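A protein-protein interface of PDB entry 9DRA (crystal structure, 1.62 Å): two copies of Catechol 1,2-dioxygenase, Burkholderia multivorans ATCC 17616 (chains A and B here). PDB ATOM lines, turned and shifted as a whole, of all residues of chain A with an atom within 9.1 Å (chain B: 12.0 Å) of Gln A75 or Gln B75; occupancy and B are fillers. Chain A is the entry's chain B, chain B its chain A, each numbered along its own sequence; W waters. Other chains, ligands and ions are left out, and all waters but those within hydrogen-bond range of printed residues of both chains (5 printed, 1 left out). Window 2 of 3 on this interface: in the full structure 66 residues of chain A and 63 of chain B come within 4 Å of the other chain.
The backbone NH (N) of Glu A78 is in hydrogen-bond range of the side-chain amide oxygen (OD1) of Asn B71 (3.3 Å).
N of Ala A79 sits at hydrogen-bond distance from OD1 of Asn B71, at 3.0 Å.
The backbone NH (N) of Glu B78 sits at hydrogen-bond distance from the side-chain amide oxygen (OD1) of Asn A71 (3.3 Å).
OD1 of Asn A71 is in hydrogen-bond range of N of Ala B79.
O of Gly B74 lies close to O of Asn A71, 3.5 Å away.
O of Gly A74 sits close to O of Asn B71.
Printed residues of chain B that touch a printed residue of chain A: Val B67, Leu B70, Asn B71, Leu B73, Gly B74, Gln B75, Gly B77, Glu B78 and Ala B79.
Hydrophobic or aromatic side chains of chain B that line the printed part of chain A: Val B67, Leu B70 and Ala B79.
Of the 14 printed residues of chain A, 8 touch a printed residue of chain B.
Of chain B, only Gly B74 and Gln B75 come within 4 Å of Gln A75.
Lys A72 touches none of the printed residues of chain B.
Leu A73 touches just one residue of chain B: Asn B71.
No residue of chain B comes within 4 Å of Asp A76.
Gly A77 touches just one residue of chain B: Asn B71.
Of the printed residues of chain B, Asn A71 touches Leu B73 (3.9 Å), Gly B74 (3.4 Å), Gly B77 (3.3 Å), Glu B78 (3.3 Å) and Ala B79 (3.0 Å).
Of the printed residues of chain A, Glu B78 touches Asn A71.
Printed residues of chain A within 4 Å of Leu B73: Asn A71 (3.9 Å).
Of the printed residues of chain A, Leu B70 touches Gly A74 (3.7 Å) and Ala A79 (3.9997 Å).
Of the printed residues of chain A, Ala B79 touches Asn A71.
Lys B72 touches none of the printed residues of chain A.
The nearest residue of chain B that does not touch Gln A75 is Asn B71 (4.6 Å).
The nearest printed residue of chain B that does not touch Ala A79 is Asn B68 (5.5 Å).
Water W1 bridges O of Leu A70 (2.7 Å) and O of Leu B70 (2.9 Å).
Water W5 bridges the side-chain amide oxygen (OE1) of Gln B75 (2.7 Å) and the backbone carbonyl oxygen (O) of Gly A74 (3.5 Å).
Water W3 lies within hydrogen-bond range of the backbone carbonyl oxygen (O) of Gly A77 (2.8 Å), the side-chain amide nitrogen (ND2) of Asn B71 (3.0 Å) and the backbone NH (N) of Ala A79 (3.3 Å).
Water W4 bridges O of Gly B74 (2.8 Å) and O of Asn A71 (3.3 Å).
Water W2 lies within hydrogen-bond range of the backbone carbonyl oxygen of Gly A74 and the backbone carbonyl oxygen of Asn B71.
Among the printed residues, merely in contact across the chains: Leu A70 with Gly B74 (3.8 Å), Asn A71 with Leu B73 (3.9 Å), Asn A71 with Gly B77 (3.3 Å), Leu A73 with Asn B71 (3.97 Å), Gly A74 with Leu B70 (3.7 Å), Gly A74 with Gly B74 (3.7 Å), Gly A74 with Gln B75 (3.6 Å), Gln A75 with Gly B74 (3.5 Å), Gln A75 with Gln B75 (3.7 Å), Gly A77 with Asn B71 (3.3 Å), Ala A79 with Val B67 (3.4 Å) and Ala A79 with Leu B70 (3.9997 Å).
Asn A71 touches Gly B77, and with the chains exchanged Gly A77 touches Asn B71.
Asn A71 touches Glu B78, and with the chains exchanged Glu A78 touches Asn B71.
Asn A71 touches Ala B79, and with the chains exchanged Ala A79 touches Asn B71.
Gly A74 touches Gln B75, and with the chains exchanged Gln A75 touches Gly B74.
Of the 18 pairs that touch across the chains among the printed residues, 16 have their exchanged pair printed and touching as well.
O of Leu B73 lies within hydrogen-bond range of N of Glu B78 (3.0 Å).
N of Ala B215 sits at hydrogen-bond distance from OE1 of Glu B78, at 3.4 Å.
OG1 of Thr B216 lies within hydrogen-bond range of OE1 of Glu B78 (2.8 Å).
The backbone carbonyl oxygen (O) of Leu A73 is in hydrogen-bond range of the backbone NH (N) of Glu A78, 3.1 Å away.
The side-chain carboxylate of Glu A78 lies within hydrogen-bond range of the backbone NH of Ala A215 (3.3 Å).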
ATOM      1  N   ASN A  68      22.783 -16.562  19.055  1.00  0.00           N
ATOM      2  CA  ASN A  68      23.185 -15.550  18.088  1.00  0.00           C
ATOM      3  C   ASN A  68      22.601 -15.873  16.732  1.00  0.00           C
ATOM      4  O   ASN A  68      22.174 -14.974  16.000  1.00  0.00           O
ATOM      5  CB  ASN A  68      24.708 -15.486  17.996  1.00  0.00           C
ATOM      6  CG  ASN A  68      25.205 -14.414  17.039  1.00  0.00           C
ATOM      7  OD1 ASN A  68      25.805 -14.711  15.999  1.00  0.00           O
ATOM      8  ND2 ASN A  68      24.982 -13.186  17.388  1.00  0.00           N
ATOM      9  N   TYR A  69      22.563 -17.159  16.389  1.00  0.00           N
ATOM     10  CA  TYR A  69      21.973 -17.551  15.115  1.00  0.00           C
ATOM     11  C   TYR A  69      20.494 -17.197  15.056  1.00  0.00           C
ATOM     12  O   TYR A  69      19.997 -16.749  14.014  1.00  0.00           O
ATOM     13  CB  TYR A  69      22.169 -19.046  14.882  1.00  0.00           C
ATOM     14  CG  TYR A  69      21.515 -19.517  13.592  1.00  0.00           C
ATOM     15  CD1 TYR A  69      22.129 -19.287  12.381  1.00  0.00           C
ATOM     16  CD2 TYR A  69      20.278 -20.144  13.610  1.00  0.00           C
ATOM     17  CE1 TYR A  69      21.535 -19.693  11.179  1.00  0.00           C
ATOM     18  CE2 TYR A  69      19.671 -20.553  12.424  1.00  0.00           C
ATOM     19  CZ  TYR A  69      20.312 -20.310  11.228  1.00  0.00           C
ATOM     20  OH  TYR A  69      19.707 -20.726  10.072  1.00  0.00           O
ATOM     21  N   LEU A  70      19.764 -17.415  16.137  1.00  0.00           N
ATOM     22  CA  LEU A  70      18.350 -17.062  16.137  1.00  0.00           C
ATOM     23  C   LEU A  70      18.170 -15.575  15.892  1.00  0.00           C
ATOM     24  O   LEU A  70      17.240 -15.165  15.184  1.00  0.00           O
ATOM     25  CB  LEU A  70      17.690 -17.463  17.450  1.00  0.00           C
ATOM     26  CG  LEU A  70      17.492 -18.948  17.724  1.00  0.00           C
ATOM     27  CD1 LEU A  70      16.727 -19.099  19.056  1.00  0.00           C
ATOM     28  CD2 LEU A  70      16.785 -19.610  16.591  1.00  0.00           C
ATOM     29  N   ASN A  71      19.048 -14.745  16.470  1.00  0.00           N
ATOM     30  CA  ASN A  71      18.969 -13.326  16.196  1.00  0.00           C
ATOM     31  C   ASN A  71      19.133 -13.058  14.700  1.00  0.00           C
ATOM     32  O   ASN A  71      18.381 -12.271  14.114  1.00  0.00           O
ATOM     33  CB  ASN A  71      20.021 -12.570  17.014  1.00  0.00           C
ATOM     34  CG  ASN A  71      19.522 -12.201  18.384  1.00  0.00           C
ATOM     35  OD1 ASN A  71      18.325 -11.947  18.587  1.00  0.00           O
ATOM     36  ND2 ASN A  71      20.447 -12.119  19.350  1.00  0.00           N
ATOM     37  N   LYS A  72      20.133 -13.691  14.077  1.00  0.00           N
ATOM     38  CA  LYS A  72      20.371 -13.464  12.653  1.00  0.00           C
ATOM     39  C   LYS A  72      19.215 -13.986  11.811  1.00  0.00           C
ATOM     40  O   LYS A  72      18.831 -13.358  10.811  1.00  0.00           O
ATOM     41  CB  LYS A  72      21.686 -14.124  12.214  1.00  0.00           C
ATOM     42  CG  LYS A  72      21.929 -13.988  10.692  1.00  0.00           C
ATOM     43  CD  LYS A  72      23.292 -14.510  10.219  1.00  0.00           C
ATOM     44  CE  LYS A  72      23.343 -14.726   8.687  1.00  0.00           C
ATOM     45  NZ  LYS A  72      22.877 -13.542   7.865  1.00  0.00           N
ATOM     46  N   LEU A  73      18.651 -15.132  12.197  1.00  0.00           N
ATOM     47  CA  LEU A  73      17.543 -15.734  11.461  1.00  0.00           C
ATOM     48  C   LEU A  73      16.367 -14.767  11.352  1.00  0.00           C
ATOM     49  O   LEU A  73      15.844 -14.520  10.252  1.00  0.00           O
ATOM     50  CB  LEU A  73      17.126 -17.025  12.161  1.00  0.00           C
ATOM     51  CG  LEU A  73      16.021 -17.849  11.485  1.00  0.00           C
ATOM     52  CD1 LEU A  73      16.474 -18.359  10.100  1.00  0.00           C
ATOM     53  CD2 LEU A  73      15.579 -19.000  12.394  1.00  0.00           C
ATOM     54  N   GLY A  74      15.943 -14.213  12.490  1.00  0.00           N
ATOM     55  CA  GLY A  74      14.837 -13.275  12.493  1.00  0.00           C
ATOM     56  C   GLY A  74      15.184 -11.937  11.867  1.00  0.00           C
ATOM     57  O   GLY A  74      14.347 -11.318  11.202  1.00  0.00           O
ATOM     58  N   GLN A  75      16.407 -11.444  12.095  1.00  0.00           N
ATOM     59  CA  GLN A  75      16.810 -10.205  11.438  1.00  0.00           C
ATOM     60  C   GLN A  75      16.740 -10.350   9.920  1.00  0.00           C
ATOM     61  O   GLN A  75      16.350  -9.414   9.220  1.00  0.00           O
ATOM     62  CB  GLN A  75      18.214  -9.784  11.874  1.00  0.00           C
ATOM     63  CG  GLN A  75      18.693  -8.456  11.263  1.00  0.00           C
ATOM     64  CD  GLN A  75      17.709  -7.297  11.467  1.00  0.00           C
ATOM     65  OE1 GLN A  75      17.238  -6.684  10.496  1.00  0.00           O
ATOM     66  NE2 GLN A  75      17.411  -6.982  12.727  1.00  0.00           N
ATOM     67  N   ASP A  76      17.109 -11.526   9.399  1.00  0.00           N
ATOM     68  CA  ASP A  76      16.989 -11.824   7.967  1.00  0.00           C
ATOM     69  C   ASP A  76      15.561 -12.095   7.529  1.00  0.00           C
ATOM     70  O   ASP A  76      15.311 -12.203   6.320  1.00  0.00           O
ATOM     71  CB  ASP A  76      17.825 -13.056   7.613  1.00  0.00           C
ATOM     72  CG  ASP A  76      19.305 -12.778   7.590  1.00  0.00           C
ATOM     73  OD1 ASP A  76      19.696 -11.596   7.621  1.00  0.00           O
ATOM     74  OD2 ASP A  76      20.084 -13.749   7.567  1.00  0.00           O
ATOM     75  N   GLY A  77      14.629 -12.238   8.460  1.00  0.00           N
ATOM     76  CA  GLY A  77      13.269 -12.610   8.093  1.00  0.00           C
ATOM     77  C   GLY A  77      13.137 -13.986   7.474  1.00  0.00           C
ATOM     78  O   GLY A  77      12.244 -14.193   6.646  1.00  0.00           O
ATOM     79  N   GLU A  78      13.980 -14.944   7.872  1.00  0.00           N
ATOM     80  CA  GLU A  78      14.086 -16.226   7.175  1.00  0.00           C
ATOM     81  C   GLU A  78      13.612 -17.429   7.970  1.00  0.00           C
ATOM     82  O   GLU A  78      13.886 -18.557   7.555  1.00  0.00           O
ATOM     83  CB  GLU A  78      15.534 -16.457   6.729  1.00  0.00           C
ATOM     84  CG  GLU A  78      15.890 -15.715   5.459  1.00  0.00           C
ATOM     85  CD  GLU A  78      17.265 -16.081   4.904  1.00  0.00           C
ATOM     86  OE1 GLU A  78      17.762 -17.198   5.172  1.00  0.00           O
ATOM     87  OE2 GLU A  78      17.846 -15.250   4.185  1.00  0.00           O
ATOM     88  N   ALA A  79      12.900 -17.253   9.091  1.00  0.00           N
ATOM     89  CA  ALA A  79      12.532 -18.433   9.868  1.00  0.00           C
ATOM     90  C   ALA A  79      11.676 -19.409   9.053  1.00  0.00           C
ATOM     91  O   ALA A  79      11.773 -20.621   9.255  1.00  0.00           O
ATOM     92  CB  ALA A  79      11.824 -18.024  11.170  1.00  0.00           C
ATOM     93  N   GLY A 214      22.230 -15.355   3.692  1.00  0.00           N
ATOM     94  CA  GLY A 214      21.216 -15.394   4.721  1.00  0.00           C
ATOM     95  C   GLY A 214      21.419 -16.530   5.692  1.00  0.00           C
ATOM     96  O   GLY A 214      22.279 -17.396   5.524  1.00  0.00           O
ATOM     97  N   ALA A 215      20.606 -16.498   6.754  1.00  0.00           N
ATOM     98  CA  ALA A 215      20.779 -17.433   7.856  1.00  0.00           C
ATOM     99  C   ALA A 215      20.501 -18.866   7.432  1.00  0.00           C
ATOM    100  O   ALA A 215      21.154 -19.791   7.928  1.00  0.00           O
ATOM    101  CB  ALA A 215      19.849 -17.043   9.001  1.00  0.00           C
ATOM    102  N   GLY B  66       4.789 -20.133  15.873  1.00  0.00           N
ATOM    103  CA  GLY B  66       6.135 -20.222  16.429  1.00  0.00           C
ATOM    104  C   GLY B  66       7.210 -19.772  15.461  1.00  0.00           C
ATOM    105  O   GLY B  66       8.156 -19.087  15.845  1.00  0.00           O
ATOM    106  N   VAL B  67       7.048 -20.092  14.173  1.00  0.00           N
ATOM    107  CA  VAL B  67       7.991 -19.612  13.175  1.00  0.00           C
ATOM    108  C   VAL B  67       7.943 -18.095  13.092  1.00  0.00           C
ATOM    109  O   VAL B  67       8.981 -17.430  12.999  1.00  0.00           O
ATOM    110  CB  VAL B  67       7.683 -20.268  11.810  1.00  0.00           C
ATOM    111  CG1 VAL B  67       8.464 -19.590  10.690  1.00  0.00           C
ATOM    112  CG2 VAL B  67       7.967 -21.743  11.894  1.00  0.00           C
ATOM    113  N   ASN B  68       6.737 -17.527  13.130  1.00  0.00           N
ATOM    114  CA  ASN B  68       6.585 -16.076  13.052  1.00  0.00           C
ATOM    115  C   ASN B  68       7.186 -15.421  14.280  1.00  0.00           C
ATOM    116  O   ASN B  68       7.791 -14.351  14.188  1.00  0.00           O
ATOM    117  CB  ASN B  68       5.102 -15.718  12.918  1.00  0.00           C
ATOM    118  CG  ASN B  68       4.862 -14.220  12.725  1.00  0.00           C
ATOM    119  OD1 ASN B  68       5.270 -13.640  11.735  1.00  0.00           O
ATOM    120  ND2 ASN B  68       4.165 -13.605  13.673  1.00  0.00           N
ATOM    121  N   TYR B  69       7.077 -16.098  15.418  1.00  0.00           N
ATOM    122  CA  TYR B  69       7.661 -15.568  16.643  1.00  0.00           C
ATOM    123  C   TYR B  69       9.174 -15.497  16.528  1.00  0.00           C
ATOM    124  O   TYR B  69       9.772 -14.489  16.917  1.00  0.00           O
ATOM    125  CB  TYR B  69       7.246 -16.407  17.834  1.00  0.00           C
ATOM    126  CG  TYR B  69       7.894 -15.907  19.102  1.00  0.00           C
ATOM    127  CD1 TYR B  69       7.413 -14.774  19.743  1.00  0.00           C
ATOM    128  CD2 TYR B  69       9.013 -16.545  19.599  1.00  0.00           C
ATOM    129  CE1 TYR B  69       8.015 -14.307  20.890  1.00  0.00           C
ATOM    130  CE2 TYR B  69       9.621 -16.087  20.758  1.00  0.00           C
ATOM    131  CZ  TYR B  69       9.120 -14.961  21.370  1.00  0.00           C
ATOM    132  OH  TYR B  69       9.742 -14.517  22.520  1.00  0.00           O
ATOM    133  N   LEU B  70       9.802 -16.535  15.963  1.00  0.00           N
ATOM    134  CA  LEU B  70      11.248 -16.504  15.745  1.00  0.00           C
ATOM    135  C   LEU B  70      11.658 -15.336  14.858  1.00  0.00           C
ATOM    136  O   LEU B  70      12.693 -14.706  15.111  1.00  0.00           O
ATOM    137  CB  LEU B  70      11.738 -17.828  15.164  1.00  0.00           C
ATOM    138  CG  LEU B  70      11.686 -19.047  16.097  1.00  0.00           C
ATOM    139  CD1 LEU B  70      12.193 -20.265  15.341  1.00  0.00           C
ATOM    140  CD2 LEU B  70      12.489 -18.845  17.374  1.00  0.00           C
ATOM    141  N   ASN B  71      10.892 -15.041  13.786  1.00  0.00           N
ATOM    142  CA  ASN B  71      11.213 -13.858  13.005  1.00  0.00           C
ATOM    143  C   ASN B  71      11.191 -12.604  13.874  1.00  0.00           C
ATOM    144  O   ASN B  71      12.114 -11.789  13.814  1.00  0.00           O
ATOM    145  CB  ASN B  71      10.269 -13.712  11.807  1.00  0.00           C
ATOM    146  CG  ASN B  71      10.687 -14.592  10.637  1.00  0.00           C
ATOM    147  OD1 ASN B  71      11.883 -14.806  10.401  1.00  0.00           O
ATOM    148  ND2 ASN B  71       9.710 -15.112   9.893  1.00  0.00           N
ATOM    149  N   LYS B  72      10.131 -12.415  14.669  1.00  0.00           N
ATOM    150  CA  LYS B  72      10.037 -11.211  15.498  1.00  0.00           C
ATOM    151  C   LYS B  72      11.141 -11.172  16.550  1.00  0.00           C
ATOM    152  O   LYS B  72      11.704 -10.111  16.830  1.00  0.00           O
ATOM    153  CB  LYS B  72       8.661 -11.138  16.170  1.00  0.00           C
ATOM    154  CG  LYS B  72       8.524  -9.979  17.167  1.00  0.00           C
ATOM    155  CD  LYS B  72       7.094  -9.783  17.684  1.00  0.00           C
ATOM    156  CE  LYS B  72       7.045  -8.841  18.927  1.00  0.00           C
ATOM    157  NZ  LYS B  72       7.724  -7.509  18.727  1.00  0.00           N
ATOM    158  N   LEU B  73      11.466 -12.329  17.133  1.00  0.00           N
ATOM    159  CA  LEU B  73      12.501 -12.413  18.164  1.00  0.00           C
ATOM    160  C   LEU B  73      13.826 -11.885  17.643  1.00  0.00           C
ATOM    161  O   LEU B  73      14.510 -11.103  18.313  1.00  0.00           O
ATOM    162  CB  LEU B  73      12.669 -13.865  18.605  1.00  0.00           C
ATOM    163  CG  LEU B  73      13.694 -14.139  19.727  1.00  0.00           C
ATOM    164  CD1 LEU B  73      13.268 -13.531  21.072  1.00  0.00           C
ATOM    165  CD2 LEU B  73      13.920 -15.663  19.863  1.00  0.00           C
ATOM    166  N   GLY B  74      14.216 -12.325  16.449  1.00  0.00           N
ATOM    167  CA  GLY B  74      15.470 -11.866  15.882  1.00  0.00           C
ATOM    168  C   GLY B  74      15.407 -10.460  15.345  1.00  0.00           C
ATOM    169  O   GLY B  74      16.396  -9.720  15.423  1.00  0.00           O
ATOM    170  N   GLN B  75      14.258 -10.064  14.791  1.00  0.00           N
ATOM    171  CA  GLN B  75      14.103  -8.687  14.330  1.00  0.00           C
ATOM    172  C   GLN B  75      14.252  -7.726  15.499  1.00  0.00           C
ATOM    173  O   GLN B  75      14.818  -6.639  15.353  1.00  0.00           O
ATOM    174  CB  GLN B  75      12.745  -8.520  13.648  1.00  0.00           C
ATOM    175  CG  GLN B  75      12.459  -7.095  13.174  1.00  0.00           C
ATOM    176  CD  GLN B  75      13.456  -6.635  12.127  1.00  0.00           C
ATOM    177  OE1 GLN B  75      13.701  -7.336  11.144  1.00  0.00           O
ATOM    178  NE2 GLN B  75      14.049  -5.458  12.340  1.00  0.00           N
ATOM    179  N   ASP B  76      13.785  -8.140  16.676  1.00  0.00           N
ATOM    180  CA  ASP B  76      13.927  -7.355  17.894  1.00  0.00           C
ATOM    181  C   ASP B  76      15.319  -7.452  18.505  1.00  0.00           C
ATOM    182  O   ASP B  76      15.629  -6.696  19.440  1.00  0.00           O
ATOM    183  CB  ASP B  76      12.900  -7.814  18.932  1.00  0.00           C
ATOM    184  CG  ASP B  76      11.475  -7.399  18.604  1.00  0.00           C
ATOM    185  OD1 ASP B  76      11.263  -6.497  17.760  1.00  0.00           O
ATOM    186  OD2 ASP B  76      10.544  -7.992  19.200  1.00  0.00           O
ATOM    187  N   GLY B  77      16.150  -8.375  18.042  1.00  0.00           N
ATOM    188  CA  GLY B  77      17.456  -8.576  18.639  1.00  0.00           C
ATOM    189  C   GLY B  77      17.398  -9.112  20.046  1.00  0.00           C
ATOM    190  O   GLY B  77      18.245  -8.771  20.872  1.00  0.00           O
ATOM    191  N   GLU B  78      16.381  -9.899  20.361  1.00  0.00           N
ATOM    192  CA  GLU B  78      16.088 -10.272  21.739  1.00  0.00           C
ATOM    193  C   GLU B  78      16.294 -11.748  22.063  1.00  0.00           C
ATOM    194  O   GLU B  78      15.901 -12.178  23.149  1.00  0.00           O
ATOM    195  CB  GLU B  78      14.645  -9.876  22.088  1.00  0.00           C
ATOM    196  CG  GLU B  78      14.465  -8.408  22.416  1.00  0.00           C
ATOM    197  CD  GLU B  78      13.089  -8.099  23.006  1.00  0.00           C
ATOM    198  OE1 GLU B  78      12.467  -8.998  23.600  1.00  0.00           O
ATOM    199  OE2 GLU B  78      12.616  -6.961  22.877  1.00  0.00           O
ATOM    200  N   ALA B  79      16.985 -12.520  21.230  1.00  0.00           N
ATOM    201  CA  ALA B  79      17.099 -13.949  21.530  1.00  0.00           C
ATOM    202  C   ALA B  79      17.815 -14.186  22.861  1.00  0.00           C
ATOM    203  O   ALA B  79      17.503 -15.147  23.568  1.00  0.00           O
ATOM    204  CB  ALA B  79      17.826 -14.687  20.425  1.00  0.00           C
ATOM    205  N   ALA B  80      18.817 -13.349  23.192  1.00  0.00           N
ATOM    206  CA  ALA B  80      19.538 -13.535  24.466  1.00  0.00           C
ATOM    207  C   ALA B  80      18.726 -13.069  25.663  1.00  0.00           C
ATOM    208  O   ALA B  80      18.923 -13.574  26.782  1.00  0.00           O
ATOM    209  CB  ALA B  80      20.876 -12.796  24.438  1.00  0.00           C
ATOM    210  N   LEU B  81      17.816 -12.121  25.462  1.00  0.00           N
ATOM    211  CA  LEU B  81      16.906 -11.734  26.536  1.00  0.00           C
ATOM    212  C   LEU B  81      15.924 -12.855  26.826  1.00  0.00           C
ATOM    213  O   LEU B  81      15.666 -13.181  27.987  1.00  0.00           O
ATOM    214  CB  LEU B  81      16.141 -10.461  26.180  1.00  0.00           C
ATOM    215  CG  LEU B  81      16.839  -9.107  26.289  1.00  0.00           C
ATOM    216  CD1 LEU B  81      17.773  -8.874  25.133  1.00  0.00           C
ATOM    217  CD2 LEU B  81      15.795  -8.009  26.380  1.00  0.00           C
ATOM    218  N   LEU B  82      15.404 -13.487  25.782  1.00  0.00           N
ATOM    219  CA  LEU B  82      14.566 -14.663  25.980  1.00  0.00           C
ATOM    220  C   LEU B  82      15.348 -15.797  26.661  1.00  0.00           C
ATOM    221  O   LEU B  82      14.825 -16.476  27.554  1.00  0.00           O
ATOM    222  CB  LEU B  82      13.995 -15.103  24.625  1.00  0.00           C
ATOM    223  CG  LEU B  82      13.164 -16.376  24.682  1.00  0.00           C
ATOM    224  CD1 LEU B  82      11.977 -16.211  25.608  1.00  0.00           C
ATOM    225  CD2 LEU B  82      12.674 -16.772  23.280  1.00  0.00           C
ATOM    226  N   PRO B 211      11.595  -4.863  27.209  1.00  0.00           N
ATOM    227  CA  PRO B 211      10.854  -3.950  26.295  1.00  0.00           C
ATOM    228  C   PRO B 211       9.412  -4.390  26.151  1.00  0.00           C
ATOM    229  O   PRO B 211       9.161  -5.519  25.715  1.00  0.00           O
ATOM    230  CB  PRO B 211      11.608  -4.084  24.963  1.00  0.00           C
ATOM    231  CG  PRO B 211      12.989  -4.496  25.345  1.00  0.00           C
ATOM    232  CD  PRO B 211      12.859  -5.335  26.611  1.00  0.00           C
ATOM    233  N   GLN B 213       6.825  -4.034  24.187  1.00  0.00           N
ATOM    234  CA  GLN B 213       6.325  -4.506  22.906  1.00  0.00           C
ATOM    235  C   GLN B 213       7.246  -5.523  22.242  1.00  0.00           C
ATOM    236  O   GLN B 213       6.969  -5.945  21.115  1.00  0.00           O
ATOM    237  CB  GLN B 213       6.111  -3.311  21.967  1.00  0.00           C
ATOM    238  CG  GLN B 213       5.199  -2.237  22.549  1.00  0.00           C
ATOM    239  CD  GLN B 213       3.877  -2.806  23.036  1.00  0.00           C
ATOM    240  OE1 GLN B 213       3.308  -3.701  22.414  1.00  0.00           O
ATOM    241  NE2 GLN B 213       3.396  -2.303  24.164  1.00  0.00           N
ATOM    242  N   GLY B 214       8.317  -5.913  22.892  1.00  0.00           N
ATOM    243  CA  GLY B 214       9.258  -6.832  22.300  1.00  0.00           C
ATOM    244  C   GLY B 214       8.842  -8.282  22.426  1.00  0.00           C
ATOM    245  O   GLY B 214       7.871  -8.629  23.109  1.00  0.00           O
ATOM    246  N   ALA B 215       9.597  -9.125  21.712  1.00  0.00           N
ATOM    247  CA  ALA B 215       9.267 -10.544  21.611  1.00  0.00           C
ATOM    248  C   ALA B 215       9.350 -11.253  22.959  1.00  0.00           C
ATOM    249  O   ALA B 215       8.545 -12.149  23.236  1.00  0.00           O
ATOM    250  CB  ALA B 215      10.194 -11.238  20.610  1.00  0.00           C
ATOM    251  N   THR B 216      10.320 -10.889  23.807  1.00  0.00           N
ATOM    252  CA  THR B 216      10.448 -11.594  25.076  1.00  0.00           C
ATOM    253  C   THR B 216       9.212 -11.377  25.934  1.00  0.00           C
ATOM    254  O   THR B 216       8.609 -12.341  26.424  1.00  0.00           O
ATOM    255  CB  THR B 216      11.717 -11.148  25.794  1.00  0.00           C
ATOM    256  OG1 THR B 216      12.840 -11.456  24.958  1.00  0.00           O
ATOM    257  CG2 THR B 216      11.909 -11.875  27.117  1.00  0.00           C
ATOM    258  N   GLN B 218       6.324 -10.498  24.902  1.00  0.00           N
ATOM    259  CA  GLN B 218       5.146 -11.091  24.281  1.00  0.00           C
ATOM    260  C   GLN B 218       4.985 -12.541  24.727  1.00  0.00           C
ATOM    261  O   GLN B 218       3.898 -12.966  25.133  1.00  0.00           O
ATOM    262  CB  GLN B 218       5.243 -10.989  22.761  1.00  0.00           C
ATOM    263  CG  GLN B 218       4.077 -11.601  22.009  1.00  0.00           C
ATOM    264  CD  GLN B 218       4.219 -11.435  20.498  1.00  0.00           C
ATOM    265  OE1 GLN B 218       3.687 -10.500  19.907  1.00  0.00           O
ATOM    266  NE2 GLN B 218       4.975 -12.313  19.889  1.00  0.00           N
HETATM  267  O   HOH W   1      14.973 -16.378  15.874  1.00  0.00           O
HETATM  268  O   HOH W   2      11.610 -10.661  10.676  1.00  0.00           O
HETATM  269  O   HOH W   3      10.440 -16.191   7.227  1.00  0.00           O
HETATM  270  O   HOH W   4      19.150  -9.340  15.519  1.00  0.00           O
HETATM  271  O   HOH W   5      12.794  -8.971   9.204  1.00  0.00           O
